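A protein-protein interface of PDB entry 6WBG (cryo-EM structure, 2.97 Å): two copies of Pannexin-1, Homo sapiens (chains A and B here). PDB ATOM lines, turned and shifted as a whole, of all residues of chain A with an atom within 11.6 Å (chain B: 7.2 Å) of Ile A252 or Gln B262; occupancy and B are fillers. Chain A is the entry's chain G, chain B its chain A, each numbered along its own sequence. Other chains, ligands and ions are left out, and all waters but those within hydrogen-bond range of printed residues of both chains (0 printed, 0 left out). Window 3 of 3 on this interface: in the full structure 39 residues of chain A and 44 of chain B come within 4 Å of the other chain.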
ATOM      1  N   GLN A  76      11.319   1.101  21.093  1.00  0.00           N
ATOM      2  CA  GLN A  76      10.290   1.629  20.205  1.00  0.00           C
ATOM      3  C   GLN A  76       8.901   1.381  20.771  1.00  0.00           C
ATOM      4  O   GLN A  76       8.025   2.251  20.703  1.00  0.00           O
ATOM      5  CB  GLN A  76      10.425   1.003  18.822  1.00  0.00           C
ATOM      6  CG  GLN A  76      11.656   1.436  18.072  1.00  0.00           C
ATOM      7  CD  GLN A  76      11.631   0.980  16.640  1.00  0.00           C
ATOM      8  OE1 GLN A  76      11.688   1.786  15.717  1.00  0.00           O
ATOM      9  NE2 GLN A  76      11.533  -0.323  16.441  1.00  0.00           N
ATOM     10  N   PHE A  79       8.370   3.795  23.467  1.00  0.00           N
ATOM     11  CA  PHE A  79       8.011   5.085  22.898  1.00  0.00           C
ATOM     12  C   PHE A  79       6.549   5.120  22.511  1.00  0.00           C
ATOM     13  O   PHE A  79       5.871   6.122  22.735  1.00  0.00           O
ATOM     14  CB  PHE A  79       8.862   5.408  21.674  1.00  0.00           C
ATOM     15  CG  PHE A  79       8.390   6.621  20.925  1.00  0.00           C
ATOM     16  CD1 PHE A  79       8.750   7.886  21.336  1.00  0.00           C
ATOM     17  CD2 PHE A  79       7.580   6.500  19.814  1.00  0.00           C
ATOM     18  CE1 PHE A  79       8.320   9.000  20.657  1.00  0.00           C
ATOM     19  CE2 PHE A  79       7.148   7.612  19.135  1.00  0.00           C
ATOM     20  CZ  PHE A  79       7.519   8.864  19.557  1.00  0.00           C
ATOM     21  N   TYR A  83       4.081   7.715  24.189  1.00  0.00           N
ATOM     22  CA  TYR A  83       3.494   8.679  23.274  1.00  0.00           C
ATOM     23  C   TYR A  83       1.984   8.651  23.364  1.00  0.00           C
ATOM     24  O   TYR A  83       1.343   9.697  23.421  1.00  0.00           O
ATOM     25  CB  TYR A  83       3.936   8.397  21.840  1.00  0.00           C
ATOM     26  CG  TYR A  83       3.541   9.470  20.844  1.00  0.00           C
ATOM     27  CD1 TYR A  83       2.215   9.666  20.484  1.00  0.00           C
ATOM     28  CD2 TYR A  83       4.495  10.270  20.251  1.00  0.00           C
ATOM     29  CE1 TYR A  83       1.857  10.633  19.582  1.00  0.00           C
ATOM     30  CE2 TYR A  83       4.146  11.243  19.345  1.00  0.00           C
ATOM     31  CZ  TYR A  83       2.824  11.417  19.015  1.00  0.00           C
ATOM     32  OH  TYR A  83       2.468  12.387  18.109  1.00  0.00           O
ATOM     33  N   SER A 247      -2.000   6.861  17.080  1.00  0.00           N
ATOM     34  CA  SER A 247      -1.170   6.928  15.890  1.00  0.00           C
ATOM     35  C   SER A 247       0.021   7.836  16.158  1.00  0.00           C
ATOM     36  O   SER A 247      -0.148   9.049  16.334  1.00  0.00           O
ATOM     37  CB  SER A 247      -1.978   7.444  14.703  1.00  0.00           C
ATOM     38  OG  SER A 247      -1.175   7.550  13.545  1.00  0.00           O
ATOM     39  N   ILE A 248       1.220   7.258  16.194  1.00  0.00           N
ATOM     40  CA  ILE A 248       2.419   8.071  16.366  1.00  0.00           C
ATOM     41  C   ILE A 248       2.917   8.488  14.987  1.00  0.00           C
ATOM     42  O   ILE A 248       3.879   7.930  14.453  1.00  0.00           O
ATOM     43  CB  ILE A 248       3.491   7.317  17.175  1.00  0.00           C
ATOM     44  CG1 ILE A 248       3.851   5.977  16.543  1.00  0.00           C
ATOM     45  CG2 ILE A 248       2.980   7.013  18.551  1.00  0.00           C
ATOM     46  CD1 ILE A 248       5.279   5.581  16.786  1.00  0.00           C
ATOM     47  N   LYS A 249       2.276   9.497  14.404  1.00  0.00           N
ATOM     48  CA  LYS A 249       2.602   9.929  13.053  1.00  0.00           C
ATOM     49  C   LYS A 249       2.612  11.443  12.921  1.00  0.00           C
ATOM     50  O   LYS A 249       2.275  11.965  11.852  1.00  0.00           O
ATOM     51  CB  LYS A 249       1.628   9.319  12.040  1.00  0.00           C
ATOM     52  CG  LYS A 249       1.584   7.803  12.062  1.00  0.00           C
ATOM     53  CD  LYS A 249       2.783   7.181  11.374  1.00  0.00           C
ATOM     54  CE  LYS A 249       2.523   7.002   9.894  1.00  0.00           C
ATOM     55  NZ  LYS A 249       3.553   6.140   9.259  1.00  0.00           N
ATOM     56  N   SER A 250       2.951  12.161  13.982  1.00  0.00           N
ATOM     57  CA  SER A 250       3.198  13.585  13.866  1.00  0.00           C
ATOM     58  C   SER A 250       4.695  13.841  13.754  1.00  0.00           C
ATOM     59  O   SER A 250       5.520  13.025  14.169  1.00  0.00           O
ATOM     60  CB  SER A 250       2.626  14.323  15.072  1.00  0.00           C
ATOM     61  OG  SER A 250       3.255  13.891  16.263  1.00  0.00           O
ATOM     62  N   GLY A 251       5.046  14.986  13.179  1.00  0.00           N
ATOM     63  CA  GLY A 251       6.449  15.300  12.995  1.00  0.00           C
ATOM     64  C   GLY A 251       7.065  14.487  11.871  1.00  0.00           C
ATOM     65  O   GLY A 251       6.413  14.149  10.885  1.00  0.00           O
ATOM     66  N   ILE A 252       8.351  14.169  12.035  1.00  0.00           N
ATOM     67  CA  ILE A 252       9.073  13.445  10.998  1.00  0.00           C
ATOM     68  C   ILE A 252       8.573  12.018  10.841  1.00  0.00           C
ATOM     69  O   ILE A 252       8.887  11.363   9.843  1.00  0.00           O
ATOM     70  CB  ILE A 252      10.580  13.451  11.291  1.00  0.00           C
ATOM     71  CG1 ILE A 252      10.887  12.560  12.491  1.00  0.00           C
ATOM     72  CG2 ILE A 252      11.061  14.860  11.550  1.00  0.00           C
ATOM     73  CD1 ILE A 252      12.351  12.442  12.792  1.00  0.00           C
ATOM     74  N   LEU A 253       7.802  11.511  11.803  1.00  0.00           N
ATOM     75  CA  LEU A 253       7.277  10.157  11.683  1.00  0.00           C
ATOM     76  C   LEU A 253       6.070  10.111  10.757  1.00  0.00           C
ATOM     77  O   LEU A 253       5.560   9.031  10.448  1.00  0.00           O
ATOM     78  CB  LEU A 253       6.906   9.614  13.059  1.00  0.00           C
ATOM     79  CG  LEU A 253       8.075   9.264  13.967  1.00  0.00           C
ATOM     80  CD1 LEU A 253       7.564   8.726  15.286  1.00  0.00           C
ATOM     81  CD2 LEU A 253       8.963   8.255  13.283  1.00  0.00           C
ATOM     82  N   ARG A 254       5.599  11.277  10.311  1.00  0.00           N
ATOM     83  CA  ARG A 254       4.340  11.342   9.574  1.00  0.00           C
ATOM     84  C   ARG A 254       4.383  10.489   8.315  1.00  0.00           C
ATOM     85  O   ARG A 254       3.510   9.646   8.092  1.00  0.00           O
ATOM     86  CB  ARG A 254       4.007  12.791   9.232  1.00  0.00           C
ATOM     87  CG  ARG A 254       2.650  12.968   8.578  1.00  0.00           C
ATOM     88  CD  ARG A 254       2.286  14.436   8.464  1.00  0.00           C
ATOM     89  NE  ARG A 254       2.117  15.056   9.775  1.00  0.00           N
ATOM     90  CZ  ARG A 254       2.962  15.934  10.302  1.00  0.00           C
ATOM     91  NH1 ARG A 254       2.728  16.447  11.502  1.00  0.00           N
ATOM     92  NH2 ARG A 254       4.044  16.301   9.629  1.00  0.00           N
ATOM     93  N   ASN A 255       5.393  10.698   7.473  1.00  0.00           N
ATOM     94  CA  ASN A 255       5.452   9.946   6.225  1.00  0.00           C
ATOM     95  C   ASN A 255       6.374   8.741   6.340  1.00  0.00           C
ATOM     96  O   ASN A 255       6.688   8.096   5.332  1.00  0.00           O
ATOM     97  CB  ASN A 255       5.878  10.863   5.080  1.00  0.00           C
ATOM     98  CG  ASN A 255       7.198  11.570   5.345  1.00  0.00           C
ATOM     99  OD1 ASN A 255       8.138  10.984   5.880  1.00  0.00           O
ATOM    100  ND2 ASN A 255       7.271  12.845   4.965  1.00  0.00           N
ATOM    101  N   ASP A 256       6.831   8.430   7.551  1.00  0.00           N
ATOM    102  CA  ASP A 256       7.629   7.232   7.768  1.00  0.00           C
ATOM    103  C   ASP A 256       6.815   5.989   7.430  1.00  0.00           C
ATOM    104  O   ASP A 256       5.592   5.976   7.573  1.00  0.00           O
ATOM    105  CB  ASP A 256       8.112   7.174   9.219  1.00  0.00           C
ATOM    106  CG  ASP A 256       9.270   6.219   9.412  1.00  0.00           C
ATOM    107  OD1 ASP A 256       9.341   5.209   8.684  1.00  0.00           O
ATOM    108  OD2 ASP A 256      10.115   6.480  10.293  1.00  0.00           O
ATOM    109  N   SER A 257       7.505   4.942   6.982  1.00  0.00           N
ATOM    110  CA  SER A 257       6.829   3.742   6.505  1.00  0.00           C
ATOM    111  C   SER A 257       6.984   2.542   7.426  1.00  0.00           C
ATOM    112  O   SER A 257       6.083   1.698   7.464  1.00  0.00           O
ATOM    113  CB  SER A 257       7.341   3.370   5.110  1.00  0.00           C
ATOM    114  OG  SER A 257       7.024   4.378   4.168  1.00  0.00           O
ATOM    115  N   THR A 258       8.089   2.439   8.162  1.00  0.00           N
ATOM    116  CA  THR A 258       8.288   1.280   9.026  1.00  0.00           C
ATOM    117  C   THR A 258       7.307   1.284  10.190  1.00  0.00           C
ATOM    118  O   THR A 258       6.954   0.226  10.719  1.00  0.00           O
ATOM    119  CB  THR A 258       9.725   1.244   9.544  1.00  0.00           C
ATOM    120  OG1 THR A 258       9.866   0.171  10.483  1.00  0.00           O
ATOM    121  CG2 THR A 258      10.088   2.553  10.225  1.00  0.00           C
ATOM    122  N   VAL A 259       6.859   2.463  10.604  1.00  0.00           N
ATOM    123  CA  VAL A 259       5.917   2.597  11.709  1.00  0.00           C
ATOM    124  C   VAL A 259       4.501   2.381  11.187  1.00  0.00           C
ATOM    125  O   VAL A 259       4.116   2.978  10.172  1.00  0.00           O
ATOM    126  CB  VAL A 259       6.079   3.959  12.404  1.00  0.00           C
ATOM    127  CG1 VAL A 259       5.923   5.093  11.415  1.00  0.00           C
ATOM    128  CG2 VAL A 259       5.077   4.098  13.523  1.00  0.00           C
ATOM    129  N   PRO A 260       3.702   1.526  11.819  1.00  0.00           N
ATOM    130  CA  PRO A 260       2.339   1.292  11.335  1.00  0.00           C
ATOM    131  C   PRO A 260       1.460   2.515  11.529  1.00  0.00           C
ATOM    132  O   PRO A 260       1.780   3.439  12.278  1.00  0.00           O
ATOM    133  CB  PRO A 260       1.853   0.120  12.190  1.00  0.00           C
ATOM    134  CG  PRO A 260       2.686   0.173  13.401  1.00  0.00           C
ATOM    135  CD  PRO A 260       4.030   0.660  12.962  1.00  0.00           C
ATOM    136  N   CYS B  66      12.076   9.001  22.384  1.00  0.00           N
ATOM    137  CA  CYS B  66      12.611   9.536  21.144  1.00  0.00           C
ATOM    138  C   CYS B  66      12.422   8.661  19.914  1.00  0.00           C
ATOM    139  O   CYS B  66      12.672   9.142  18.806  1.00  0.00           O
ATOM    140  CB  CYS B  66      14.104   9.842  21.305  1.00  0.00           C
ATOM    141  SG  CYS B  66      14.413  11.424  22.095  1.00  0.00           S
ATOM    142  N   PHE B  67      11.993   7.412  20.064  1.00  0.00           N
ATOM    143  CA  PHE B  67      11.750   6.540  18.919  1.00  0.00           C
ATOM    144  C   PHE B  67      12.959   6.402  18.006  1.00  0.00           C
ATOM    145  O   PHE B  67      12.957   6.906  16.880  1.00  0.00           O
ATOM    146  CB  PHE B  67      10.558   7.015  18.090  1.00  0.00           C
ATOM    147  CG  PHE B  67      10.076   5.990  17.112  1.00  0.00           C
ATOM    148  CD1 PHE B  67       9.404   4.869  17.549  1.00  0.00           C
ATOM    149  CD2 PHE B  67      10.323   6.128  15.764  1.00  0.00           C
ATOM    150  CE1 PHE B  67       8.976   3.920  16.664  1.00  0.00           C
ATOM    151  CE2 PHE B  67       9.899   5.174  14.878  1.00  0.00           C
ATOM    152  CZ  PHE B  67       9.227   4.071  15.331  1.00  0.00           C
ATOM    153  N   PRO B  69      15.445   4.140  15.563  1.00  0.00           N
ATOM    154  CA  PRO B  69      15.089   3.100  14.596  1.00  0.00           C
ATOM    155  C   PRO B  69      15.105   1.718  15.227  1.00  0.00           C
ATOM    156  O   PRO B  69      15.607   1.509  16.334  1.00  0.00           O
ATOM    157  CB  PRO B  69      16.173   3.223  13.522  1.00  0.00           C
ATOM    158  CG  PRO B  69      16.666   4.600  13.650  1.00  0.00           C
ATOM    159  CD  PRO B  69      16.601   4.924  15.106  1.00  0.00           C
ATOM    160  N   SER B  93      21.175  21.451  18.152  1.00  0.00           N
ATOM    161  CA  SER B  93      20.865  20.047  17.899  1.00  0.00           C
ATOM    162  C   SER B  93      19.400  19.850  17.538  1.00  0.00           C
ATOM    163  O   SER B  93      19.080  19.113  16.599  1.00  0.00           O
ATOM    164  CB  SER B  93      21.229  19.204  19.121  1.00  0.00           C
ATOM    165  OG  SER B  93      22.602  19.335  19.443  1.00  0.00           O
ATOM    166  N   GLN B  95      15.445  20.858  16.464  1.00  0.00           N
ATOM    167  CA  GLN B  95      14.641  21.744  15.634  1.00  0.00           C
ATOM    168  C   GLN B  95      13.178  21.553  16.006  1.00  0.00           C
ATOM    169  O   GLN B  95      12.616  20.475  15.783  1.00  0.00           O
ATOM    170  CB  GLN B  95      14.865  21.460  14.150  1.00  0.00           C
ATOM    171  N   GLU B 243       6.670  17.905  21.227  1.00  0.00           N
ATOM    172  CA  GLU B 243       7.277  17.077  20.199  1.00  0.00           C
ATOM    173  C   GLU B 243       8.331  17.897  19.480  1.00  0.00           C
ATOM    174  O   GLU B 243       8.009  18.889  18.819  1.00  0.00           O
ATOM    175  CB  GLU B 243       6.235  16.576  19.203  1.00  0.00           C
ATOM    176  CG  GLU B 243       5.174  15.703  19.816  1.00  0.00           C
ATOM    177  CD  GLU B 243       4.325  15.027  18.771  1.00  0.00           C
ATOM    178  OE1 GLU B 243       4.673  15.121  17.578  1.00  0.00           O
ATOM    179  OE2 GLU B 243       3.311  14.401  19.139  1.00  0.00           O
ATOM    180  N   PHE B 244       9.585  17.487  19.611  1.00  0.00           N
ATOM    181  CA  PHE B 244      10.672  18.199  18.970  1.00  0.00           C
ATOM    182  C   PHE B 244      11.545  17.199  18.239  1.00  0.00           C
ATOM    183  O   PHE B 244      11.685  16.050  18.658  1.00  0.00           O
ATOM    184  CB  PHE B 244      11.496  18.998  19.980  1.00  0.00           C
ATOM    185  CG  PHE B 244      12.230  18.151  20.974  1.00  0.00           C
ATOM    186  CD1 PHE B 244      11.557  17.508  21.991  1.00  0.00           C
ATOM    187  CD2 PHE B 244      13.599  18.014  20.897  1.00  0.00           C
ATOM    188  CE1 PHE B 244      12.236  16.742  22.905  1.00  0.00           C
ATOM    189  CE2 PHE B 244      14.280  17.251  21.808  1.00  0.00           C
ATOM    190  CZ  PHE B 244      13.597  16.615  22.811  1.00  0.00           C
ATOM    191  N   VAL B 245      12.119  17.647  17.134  1.00  0.00           N
ATOM    192  CA  VAL B 245      13.007  16.822  16.332  1.00  0.00           C
ATOM    193  C   VAL B 245      14.417  17.017  16.860  1.00  0.00           C
ATOM    194  O   VAL B 245      14.873  18.150  17.029  1.00  0.00           O
ATOM    195  CB  VAL B 245      12.913  17.189  14.847  1.00  0.00           C
ATOM    196  CG1 VAL B 245      13.693  16.208  14.023  1.00  0.00           C
ATOM    197  CG2 VAL B 245      11.466  17.220  14.413  1.00  0.00           C
ATOM    198  N   CYS B 246      15.108  15.917  17.123  1.00  0.00           N
ATOM    199  CA  CYS B 246      16.417  15.936  17.755  1.00  0.00           C
ATOM    200  C   CYS B 246      17.396  15.150  16.899  1.00  0.00           C
ATOM    201  O   CYS B 246      17.032  14.123  16.320  1.00  0.00           O
ATOM    202  CB  CYS B 246      16.341  15.351  19.162  1.00  0.00           C
ATOM    203  SG  CYS B 246      17.906  14.833  19.861  1.00  0.00           S
ATOM    204  N   SER B 247      18.627  15.636  16.817  1.00  0.00           N
ATOM    205  CA  SER B 247      19.636  15.061  15.943  1.00  0.00           C
ATOM    206  C   SER B 247      20.911  14.818  16.738  1.00  0.00           C
ATOM    207  O   SER B 247      21.565  15.772  17.172  1.00  0.00           O
ATOM    208  CB  SER B 247      19.912  15.991  14.764  1.00  0.00           C
ATOM    209  OG  SER B 247      20.918  15.464  13.923  1.00  0.00           O
ATOM    210  N   ILE B 248      21.263  13.549  16.932  1.00  0.00           N
ATOM    211  CA  ILE B 248      22.512  13.233  17.613  1.00  0.00           C
ATOM    212  C   ILE B 248      23.618  13.137  16.569  1.00  0.00           C
ATOM    213  O   ILE B 248      24.044  12.048  16.177  1.00  0.00           O
ATOM    214  CB  ILE B 248      22.380  11.944  18.448  1.00  0.00           C
ATOM    215  CG1 ILE B 248      21.928  10.758  17.606  1.00  0.00           C
ATOM    216  CG2 ILE B 248      21.345  12.125  19.517  1.00  0.00           C
ATOM    217  CD1 ILE B 248      22.474   9.447  18.098  1.00  0.00           C
ATOM    218  N   LYS B 249      24.114  14.287  16.124  1.00  0.00           N
ATOM    219  CA  LYS B 249      25.112  14.331  15.063  1.00  0.00           C
ATOM    220  C   LYS B 249      26.198  15.357  15.338  1.00  0.00           C
ATOM    221  O   LYS B 249      26.733  15.949  14.393  1.00  0.00           O
ATOM    222  CB  LYS B 249      24.451  14.612  13.711  1.00  0.00           C
ATOM    223  CG  LYS B 249      23.382  13.607  13.323  1.00  0.00           C
ATOM    224  CD  LYS B 249      23.970  12.300  12.834  1.00  0.00           C
ATOM    225  CE  LYS B 249      24.226  12.348  11.344  1.00  0.00           C
ATOM    226  NZ  LYS B 249      24.525  11.001  10.795  1.00  0.00           N
ATOM    227  N   VAL B 259      23.620   6.090  11.945  1.00  0.00           N
ATOM    228  CA  VAL B 259      22.707   6.882  12.764  1.00  0.00           C
ATOM    229  C   VAL B 259      21.856   7.762  11.855  1.00  0.00           C
ATOM    230  O   VAL B 259      22.392   8.438  10.967  1.00  0.00           O
ATOM    231  CB  VAL B 259      23.484   7.703  13.807  1.00  0.00           C
ATOM    232  CG1 VAL B 259      24.521   8.582  13.143  1.00  0.00           C
ATOM    233  CG2 VAL B 259      22.533   8.543  14.624  1.00  0.00           C
ATOM    234  N   PRO B 260      20.535   7.766  12.014  1.00  0.00           N
ATOM    235  CA  PRO B 260      19.691   8.594  11.150  1.00  0.00           C
ATOM    236  C   PRO B 260      19.896  10.075  11.420  1.00  0.00           C
ATOM    237  O   PRO B 260      20.453  10.482  12.440  1.00  0.00           O
ATOM    238  CB  PRO B 260      18.271   8.158  11.512  1.00  0.00           C
ATOM    239  CG  PRO B 260      18.388   7.599  12.869  1.00  0.00           C
ATOM    240  CD  PRO B 260      19.734   6.948  12.936  1.00  0.00           C
ATOM    241  N   ASP B 261      19.423  10.884  10.474  1.00  0.00           N
ATOM    242  CA  ASP B 261      19.682  12.318  10.531  1.00  0.00           C
ATOM    243  C   ASP B 261      19.009  12.963  11.731  1.00  0.00           C
ATOM    244  O   ASP B 261      19.584  13.849  12.371  1.00  0.00           O
ATOM    245  CB  ASP B 261      19.225  12.984   9.240  1.00  0.00           C
ATOM    246  CG  ASP B 261      20.099  12.622   8.062  1.00  0.00           C
ATOM    247  OD1 ASP B 261      21.299  12.360   8.276  1.00  0.00           O
ATOM    248  OD2 ASP B 261      19.588  12.599   6.923  1.00  0.00           O
ATOM    249  N   GLN B 262      17.794  12.536  12.058  1.00  0.00           N
ATOM    250  CA  GLN B 262      17.037  13.175  13.120  1.00  0.00           C
ATOM    251  C   GLN B 262      16.053  12.190  13.727  1.00  0.00           C
ATOM    252  O   GLN B 262      15.590  11.260  13.066  1.00  0.00           O
ATOM    253  CB  GLN B 262      16.297  14.402  12.601  1.00  0.00           C
ATOM    254  CG  GLN B 262      15.528  14.160  11.326  1.00  0.00           C
ATOM    255  CD  GLN B 262      15.051  15.447  10.699  1.00  0.00           C
ATOM    256  OE1 GLN B 262      15.556  16.524  11.009  1.00  0.00           O
ATOM    257  NE2 GLN B 262      14.069  15.346   9.814  1.00  0.00           N
ATOM    258  N   PHE B 263      15.735  12.416  14.996  1.00  0.00           N
ATOM    259  CA  PHE B 263      14.836  11.563  15.755  1.00  0.00           C
ATOM    260  C   PHE B 263      13.612  12.357  16.177  1.00  0.00           C
ATOM    261  O   PHE B 263      13.707  13.553  16.458  1.00  0.00           O
ATOM    262  CB  PHE B 263      15.525  11.002  16.992  1.00  0.00           C
ATOM    263  CG  PHE B 263      16.700  10.136  16.684  1.00  0.00           C
ATOM    264  CD1 PHE B 263      17.923  10.687  16.376  1.00  0.00           C
ATOM    265  CD2 PHE B 263      16.582   8.765  16.713  1.00  0.00           C
ATOM    266  CE1 PHE B 263      18.999   9.890  16.093  1.00  0.00           C
ATOM    267  CE2 PHE B 263      17.656   7.967  16.433  1.00  0.00           C
ATOM    268  CZ  PHE B 263      18.865   8.531  16.127  1.00  0.00           C
ATOM    269  N   GLN B 264      12.466  11.689  16.224  1.00  0.00           N
ATOM    270  CA  GLN B 264      11.227  12.324  16.666  1.00  0.00           C
ATOM    271  C   GLN B 264      11.064  12.052  18.152  1.00  0.00           C
ATOM    272  O   GLN B 264      10.628  10.982  18.566  1.00  0.00           O
ATOM    273  CB  GLN B 264      10.037  11.807  15.874  1.00  0.00           C
ATOM    274  CG  GLN B 264       8.707  12.314  16.380  1.00  0.00           C
ATOM    275  CD  GLN B 264       8.556  13.800  16.193  1.00  0.00           C
ATOM    276  OE1 GLN B 264       8.849  14.336  15.128  1.00  0.00           O
ATOM    277  NE2 GLN B 264       8.097  14.482  17.231  1.00  0.00           N
ATOM    278  N   CYS B 265      11.421  13.036  18.967  1.00  0.00           N
ATOM    279  CA  CYS B 265      11.275  12.922  20.409  1.00  0.00           C
ATOM    280  C   CYS B 265      10.007  13.617  20.867  1.00  0.00           C
ATOM    281  O   CYS B 265       9.539  14.563  20.231  1.00  0.00           O
ATOM    282  CB  CYS B 265      12.487  13.524  21.116  1.00  0.00           C
ATOM    283  SG  CYS B 265      14.034  12.776  20.629  1.00  0.00           S
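The side-chain amide oxygen (OE1) of Gln B264 is in hydrogen-bond range of the backbone NH (N) of Ile A252, 3.1 Å away.
OE2 of Glu B243 is in hydrogen-bond range of OG of Ser A250 (2.9 Å).
OH of Tyr A83 is in hydrogen-bond range of OE2 of Glu B243, at 2.4 Å.
OG of Ser A250 sits at hydrogen-bond distance from OH of Tyr A83, 2.5 Å away.
The backbone carbonyl oxygen (O) of Gly A251 sits close to the guanidinium group (NH2) of Arg A254, at 3.4 Å.
The backbone carbonyl oxygen (O) of Val B245 lies within hydrogen-bond range of the backbone NH (N) of Gln B95, 2.8 Å away.
O of Cys B246 sits at hydrogen-bond distance from N of Phe B263, 2.5 Å away.
The side-chain sulfur (SG) of Cys B66 is disulfide-bonded to the side-chain sulfur (SG) of Cys B265, at 2.0 Å.
Among the printed residues, pairs that only touch across the chains: Gln A76 with Phe B67 (3.4 Å), Gln A76 with Pro B69 (3.5 Å), Phe A79 with Cys B66 (3.7 Å), Phe A79 with Phe B67 (3.3 Å), Phe A79 with Gln B264 (3.7 Å), Ser A250 with Gln B264 (3.7 Å), Gly A251 with Gln B264 (3.4 Å), Ile A252 with Val B245 (3.7 Å), Ile A252 with Gln B262 (3.5 Å), Ile A252 with Phe B263 (3.6 Å), Leu A253 with Phe B67 (3.5 Å) and Leu A253 with Gln B264 (3.7 Å).
Printed residues of chain B within 4 Å of Phe A79: Cys B66 (3.7 Å), Phe B67 (3.3 Å) and Gln B264 (3.7 Å).
Ile A252 touches just these residues of chain B: Val B245, Gln B262, Phe B263 and Gln B264.
Ser A257 touches none of the printed residues of chain B.
No residue of chain A comes within 4 Å of Gln B95.
Of the printed residues of chain A, Glu B243 touches Tyr A83 and Ser A250.
Of the printed residues of chain A, Val B245 touches Ile A252 (3.7 Å).
No residue of chain A comes within 4 Å of Cys B246.
No residue of chain A comes within 4 Å of Ser B247.
No residue of chain A comes within 4 Å of Pro B260.
No residue of chain A comes within 4 Å of Asp B261.
Of chain A, only Ile A252 comes within 4 Å of Gln B262.
Phe B263 touches one residue of chain A.
The nearest residue of chain A that does not touch Gln B262 is Leu A253 (7.3 Å).
The nearest printed residue of chain B that does not touch Ser A250 is Val B245 (7.3 Å).
Hydrophobic or aromatic side chains of chain B that line the printed part of chain A: Phe B67 and Val B245.
Hydrophobic or aromatic side chains of chain A that line the printed part of chain B: Phe A79, Tyr A83, Ile A252 and Leu A253.
Among the printed residues, 15 pairs touch across the chains.
Among the printed residues, no Asp or Glu carboxylate lies within 4 Å of a Lys or Arg side-chain nitrogen of the other chain.
Positions printed for both chains: 247, 248, 249, 259 and 260.
Of the 15 pairs that touch across the chains among the printed residues, none has its exchanged pair printed and touching as well.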
